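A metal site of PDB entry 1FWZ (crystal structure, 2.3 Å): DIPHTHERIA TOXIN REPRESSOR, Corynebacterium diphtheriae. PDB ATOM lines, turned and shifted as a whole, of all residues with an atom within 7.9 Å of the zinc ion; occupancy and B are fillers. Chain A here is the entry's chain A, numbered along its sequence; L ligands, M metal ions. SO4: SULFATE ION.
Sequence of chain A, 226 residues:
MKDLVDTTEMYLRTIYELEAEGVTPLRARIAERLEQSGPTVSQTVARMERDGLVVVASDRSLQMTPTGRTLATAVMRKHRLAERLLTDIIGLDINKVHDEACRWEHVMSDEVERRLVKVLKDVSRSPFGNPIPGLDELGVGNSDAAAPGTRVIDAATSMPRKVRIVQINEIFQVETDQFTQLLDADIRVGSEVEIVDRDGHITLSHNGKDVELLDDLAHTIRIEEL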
ATOM      1  N   ARG A  13      -5.595  -5.596   0.093  1.00  0.00           N
ATOM      2  CA  ARG A  13      -6.671  -5.671   1.090  1.00  0.00           C
ATOM      3  C   ARG A  13      -6.179  -5.151   2.428  1.00  0.00           C
ATOM      4  O   ARG A  13      -6.982  -4.667   3.240  1.00  0.00           O
ATOM      5  CB  ARG A  13      -7.271  -7.093   1.213  1.00  0.00           C
ATOM      6  CG  ARG A  13      -6.317  -8.199   1.665  1.00  0.00           C
ATOM      7  CD  ARG A  13      -6.532  -8.608   3.103  1.00  0.00           C
ATOM      8  NE  ARG A  13      -7.861  -9.172   3.287  1.00  0.00           N
ATOM      9  CZ  ARG A  13      -8.619  -8.964   4.363  1.00  0.00           C
ATOM     10  NH1 ARG A  13      -8.175  -8.209   5.362  1.00  0.00           N
ATOM     11  NH2 ARG A  13      -9.832  -9.509   4.434  1.00  0.00           N
ATOM     12  N   GLU A  17      -7.845  -2.164   4.521  1.00  0.00           N
ATOM     13  CA  GLU A  17      -8.233  -2.282   5.939  1.00  0.00           C
ATOM     14  C   GLU A  17      -7.795  -1.104   6.781  1.00  0.00           C
ATOM     15  O   GLU A  17      -8.616  -0.514   7.479  1.00  0.00           O
ATOM     16  CB  GLU A  17      -7.618  -3.526   6.553  1.00  0.00           C
ATOM     17  CG  GLU A  17      -8.471  -4.738   6.462  1.00  0.00           C
ATOM     18  CD  GLU A  17      -7.918  -5.863   7.300  1.00  0.00           C
ATOM     19  OE1 GLU A  17      -6.693  -6.122   7.231  1.00  0.00           O
ATOM     20  OE2 GLU A  17      -8.715  -6.483   8.030  1.00  0.00           O
ATOM     21  N   MET A  76     -12.193  -7.644  -0.644  1.00  0.00           N
ATOM     22  CA  MET A  76     -12.932  -7.462   0.625  1.00  0.00           C
ATOM     23  C   MET A  76     -14.375  -7.874   0.496  1.00  0.00           C
ATOM     24  O   MET A  76     -15.000  -8.309   1.469  1.00  0.00           O
ATOM     25  CB  MET A  76     -12.885  -6.004   1.138  1.00  0.00           C
ATOM     26  CG  MET A  76     -11.505  -5.474   1.491  1.00  0.00           C
ATOM     27  SD  MET A  76     -10.738  -6.234   2.923  1.00  0.00           S
ATOM     28  CE  MET A  76     -12.219  -6.621   3.888  1.00  0.00           C
ATOM     29  N   HIS A  79     -14.170 -11.603   0.347  1.00  0.00           N
ATOM     30  CA  HIS A  79     -13.877 -11.925   1.745  1.00  0.00           C
ATOM     31  C   HIS A  79     -15.107 -11.852   2.644  1.00  0.00           C
ATOM     32  O   HIS A  79     -15.377 -12.777   3.389  1.00  0.00           O
ATOM     33  CB  HIS A  79     -12.797 -10.978   2.301  1.00  0.00           C
ATOM     34  CG  HIS A  79     -12.547 -11.135   3.769  1.00  0.00           C
ATOM     35  ND1 HIS A  79     -11.604 -12.000   4.250  1.00  0.00           N
ATOM     36  CD2 HIS A  79     -13.144 -10.513   4.812  1.00  0.00           C
ATOM     37  CE1 HIS A  79     -11.658 -11.878   5.581  1.00  0.00           C
ATOM     38  NE2 HIS A  79     -12.559 -10.999   5.964  1.00  0.00           N
ATOM     39  N   ARG A  80     -15.877 -10.773   2.553  1.00  0.00           N
ATOM     40  CA  ARG A  80     -17.041 -10.597   3.431  1.00  0.00           C
ATOM     41  C   ARG A  80     -18.260 -11.424   3.046  1.00  0.00           C
ATOM     42  O   ARG A  80     -19.076 -11.818   3.890  1.00  0.00           O
ATOM     43  CB  ARG A  80     -17.385  -9.103   3.589  1.00  0.00           C
ATOM     44  CG  ARG A  80     -16.285  -8.338   4.270  1.00  0.00           C
ATOM     45  CD  ARG A  80     -16.522  -6.843   4.442  1.00  0.00           C
ATOM     46  NE  ARG A  80     -15.419  -6.359   5.256  1.00  0.00           N
ATOM     47  CZ  ARG A  80     -15.039  -5.086   5.387  1.00  0.00           C
ATOM     48  NH1 ARG A  80     -15.678  -4.120   4.754  1.00  0.00           N
ATOM     49  NH2 ARG A  80     -13.935  -4.830   6.093  1.00  0.00           N
ATOM     50  N   GLU A  83     -17.579 -14.839   4.503  1.00  0.00           N
ATOM     51  CA  GLU A  83     -17.887 -14.887   5.941  1.00  0.00           C
ATOM     52  C   GLU A  83     -19.369 -15.032   6.169  1.00  0.00           C
ATOM     53  O   GLU A  83     -19.804 -15.719   7.071  1.00  0.00           O
ATOM     54  CB  GLU A  83     -17.384 -13.627   6.660  1.00  0.00           C
ATOM     55  CG  GLU A  83     -15.894 -13.466   6.693  1.00  0.00           C
ATOM     56  CD  GLU A  83     -15.493 -12.201   7.376  1.00  0.00           C
ATOM     57  OE1 GLU A  83     -16.143 -11.152   7.125  1.00  0.00           O
ATOM     58  OE2 GLU A  83     -14.539 -12.232   8.180  1.00  0.00           O
ATOM     59  N   VAL A  97     -14.219 -18.101  11.358  1.00  0.00           N
ATOM     60  CA  VAL A  97     -14.753 -17.470  10.147  1.00  0.00           C
ATOM     61  C   VAL A  97     -13.845 -16.470   9.419  1.00  0.00           C
ATOM     62  O   VAL A  97     -13.788 -16.486   8.193  1.00  0.00           O
ATOM     63  CB  VAL A  97     -16.166 -16.872  10.418  1.00  0.00           C
ATOM     64  CG1 VAL A  97     -16.638 -16.070   9.240  1.00  0.00           C
ATOM     65  CG2 VAL A  97     -17.147 -17.984  10.703  1.00  0.00           C
ATOM     66  N   HIS A  98     -13.102 -15.633  10.154  1.00  0.00           N
ATOM     67  CA  HIS A  98     -12.214 -14.639   9.516  1.00  0.00           C
ATOM     68  C   HIS A  98     -11.011 -15.316   8.850  1.00  0.00           C
ATOM     69  O   HIS A  98     -10.695 -15.009   7.699  1.00  0.00           O
ATOM     70  CB  HIS A  98     -11.748 -13.568  10.546  1.00  0.00           C
ATOM     71  CG  HIS A  98     -10.846 -12.495   9.959  1.00  0.00           C
ATOM     72  ND1 HIS A  98     -11.294 -11.579   9.065  1.00  0.00           N
ATOM     73  CD2 HIS A  98      -9.496 -12.385  10.070  1.00  0.00           C
ATOM     74  CE1 HIS A  98     -10.234 -10.920   8.628  1.00  0.00           C
ATOM     75  NE2 HIS A  98      -9.120 -11.376   9.202  1.00  0.00           N
ATOM     76  N   ASP A  99     -10.366 -16.244   9.568  1.00  0.00           N
ATOM     77  CA  ASP A  99      -9.201 -16.963   9.072  1.00  0.00           C
ATOM     78  C   ASP A  99      -9.507 -17.701   7.793  1.00  0.00           C
ATOM     79  O   ASP A  99      -8.746 -17.657   6.853  1.00  0.00           O
ATOM     80  CB  ASP A  99      -8.731 -17.979  10.093  1.00  0.00           C
ATOM     81  CG  ASP A  99      -8.472 -17.361  11.415  1.00  0.00           C
ATOM     82  OD1 ASP A  99      -7.998 -16.200  11.413  1.00  0.00           O
ATOM     83  OD2 ASP A  99      -8.777 -17.990  12.460  1.00  0.00           O
ATOM     84  N   GLU A 100     -10.634 -18.393   7.808  1.00  0.00           N
ATOM     85  CA  GLU A 100     -11.090 -19.149   6.673  1.00  0.00           C
ATOM     86  C   GLU A 100     -11.367 -18.218   5.510  1.00  0.00           C
ATOM     87  O   GLU A 100     -10.852 -18.430   4.413  1.00  0.00           O
ATOM     88  CB  GLU A 100     -12.355 -19.927   7.057  1.00  0.00           C
ATOM     89  CG  GLU A 100     -12.874 -20.903   5.983  1.00  0.00           C
ATOM     90  CD  GLU A 100     -12.257 -22.298   6.058  1.00  0.00           C
ATOM     91  OE1 GLU A 100     -11.768 -22.651   7.135  1.00  0.00           O
ATOM     92  OE2 GLU A 100     -12.286 -23.047   5.065  1.00  0.00           O
ATOM     93  N   ALA A 101     -12.128 -17.152   5.746  1.00  0.00           N
ATOM     94  CA  ALA A 101     -12.466 -16.174   4.699  1.00  0.00           C
ATOM     95  C   ALA A 101     -11.227 -15.503   4.109  1.00  0.00           C
ATOM     96  O   ALA A 101     -11.237 -15.110   2.933  1.00  0.00           O
ATOM     97  CB  ALA A 101     -13.424 -15.140   5.218  1.00  0.00           C
ATOM     98  N   CSS A 102     -10.154 -15.431   4.899  1.00  0.00           N
ATOM     99  CA  CSS A 102      -8.905 -14.822   4.449  1.00  0.00           C
ATOM    100  CB  CSS A 102      -7.886 -14.701   5.591  1.00  0.00           C
ATOM    101  SG  CSS A 102      -8.271 -13.402   6.813  1.00  0.00           S
ATOM    102  SD  CSS A 102      -7.358 -11.749   6.035  1.00  0.00           S
ATOM    103  C   CSS A 102      -8.304 -15.593   3.308  1.00  0.00           C
ATOM    104  O   CSS A 102      -7.572 -15.053   2.487  1.00  0.00           O
ATOM    105  N   GLU A 105     -11.201 -15.594  -0.015  1.00  0.00           N
ATOM    106  CA  GLU A 105     -11.269 -14.340  -0.756  1.00  0.00           C
ATOM    107  C   GLU A 105     -10.419 -14.385  -2.015  1.00  0.00           C
ATOM    108  O   GLU A 105     -10.663 -13.642  -2.961  1.00  0.00           O
ATOM    109  CB  GLU A 105     -10.864 -13.163   0.117  1.00  0.00           C
ATOM    110  CG  GLU A 105      -9.398 -13.144   0.449  1.00  0.00           C
ATOM    111  CD  GLU A 105      -9.018 -12.063   1.430  1.00  0.00           C
ATOM    112  OE1 GLU A 105      -9.821 -11.762   2.363  1.00  0.00           O
ATOM    113  OE2 GLU A 105      -7.888 -11.545   1.299  1.00  0.00           O
ATOM    114  N   SER A 126     -20.651  -7.569   7.052  1.00  0.00           N
ATOM    115  CA  SER A 126     -19.982  -8.823   7.325  1.00  0.00           C
ATOM    116  C   SER A 126     -20.462  -9.160   8.728  1.00  0.00           C
ATOM    117  O   SER A 126     -20.930  -8.287   9.442  1.00  0.00           O
ATOM    118  CB  SER A 126     -18.478  -8.626   7.344  1.00  0.00           C
ATOM    119  OG  SER A 126     -18.056  -8.259   8.624  1.00  0.00           O
ATOM    120  N   PRO A 127     -20.264 -10.410   9.197  1.00  0.00           N
ATOM    121  CA  PRO A 127     -20.710 -10.802  10.542  1.00  0.00           C
ATOM    122  C   PRO A 127     -19.992  -9.989  11.633  1.00  0.00           C
ATOM    123  O   PRO A 127     -20.379  -9.994  12.814  1.00  0.00           O
ATOM    124  CB  PRO A 127     -20.310 -12.290  10.618  1.00  0.00           C
ATOM    125  CG  PRO A 127     -20.094 -12.732   9.161  1.00  0.00           C
ATOM    126  CD  PRO A 127     -19.485 -11.498   8.551  1.00  0.00           C
ATOM    127  N   PHE A 128     -18.927  -9.300  11.235  1.00  0.00           N
ATOM    128  CA  PHE A 128     -18.152  -8.518  12.161  1.00  0.00           C
ATOM    129  C   PHE A 128     -18.415  -7.009  12.107  1.00  0.00           C
ATOM    130  O   PHE A 128     -17.590  -6.229  12.555  1.00  0.00           O
ATOM    131  CB  PHE A 128     -16.665  -8.819  11.955  1.00  0.00           C
ATOM    132  CG  PHE A 128     -16.339 -10.279  11.994  1.00  0.00           C
ATOM    133  CD1 PHE A 128     -16.629 -11.029  13.129  1.00  0.00           C
ATOM    134  CD2 PHE A 128     -15.798 -10.915  10.887  1.00  0.00           C
ATOM    135  CE1 PHE A 128     -16.380 -12.403  13.150  1.00  0.00           C
ATOM    136  CE2 PHE A 128     -15.554 -12.275  10.892  1.00  0.00           C
ATOM    137  CZ  PHE A 128     -15.844 -13.025  12.026  1.00  0.00           C
ATOM    138  N   ASN A 130     -18.707  -4.826   9.521  1.00  0.00           N
ATOM    139  CA  ASN A 130     -18.220  -3.988   8.433  1.00  0.00           C
ATOM    140  C   ASN A 130     -19.048  -4.136   7.165  1.00  0.00           C
ATOM    141  O   ASN A 130     -19.496  -5.211   6.851  1.00  0.00           O
ATOM    142  CB  ASN A 130     -16.777  -4.292   8.130  1.00  0.00           C
ATOM    143  CG  ASN A 130     -15.878  -3.937   9.275  1.00  0.00           C
ATOM    144  OD1 ASN A 130     -15.359  -4.821   9.965  1.00  0.00           O
ATOM    145  ND2 ASN A 130     -15.746  -2.653   9.543  1.00  0.00           N
HETATM  146  S   SO4 L   1     -13.962  -8.123   8.362  1.00  0.00           S
HETATM  147  O1  SO4 L   1     -13.447  -7.642   7.044  1.00  0.00           O
HETATM  148  O2  SO4 L   1     -15.462  -8.016   8.376  1.00  0.00           O
HETATM  149  O3  SO4 L   1     -13.528  -9.537   8.611  1.00  0.00           O
HETATM  150  O4  SO4 L   1     -13.410  -7.241   9.442  1.00  0.00           O
HETATM  151 ZN    ZN M   1     -12.798 -11.115   8.128  1.00  0.00          ZN
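SG of CSS 102 is in hydrogen-bond range of a ring nitrogen (NE2) of His 98 (3.2 Å). The guanidinium group (NH2) of Arg 13 is in hydrogen-bond range of a ring nitrogen (ND1) of His 79 (3.1 Å). The backbone carbonyl oxygen of Ala 101 lies within hydrogen-bond range of a ring nitrogen (ND1) of His 79, at 3.4 Å. ND1 of His 79 is in hydrogen-bond range of OE1 of Glu 105, at 2.6 Å.
Three residues have an atom within 4 Å of the zinc ion: His 79, Glu 83 and His 98. Along chain A the residues within 4 Å of the zinc ion span positions 79 to 98. The nearest printed residue that does not touch the zinc ion is Phe 128 (4.1 Å).
O3 of the ligand is bound to the zinc ion (1.8 Å). The zinc ion is bound by ND1 of His 98 (1.8 Å). OE2 of Glu 83 is bound to the zinc ion, 2.1 Å away. The zinc ion is bound by NE2 of His 79, at 2.2 Å.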
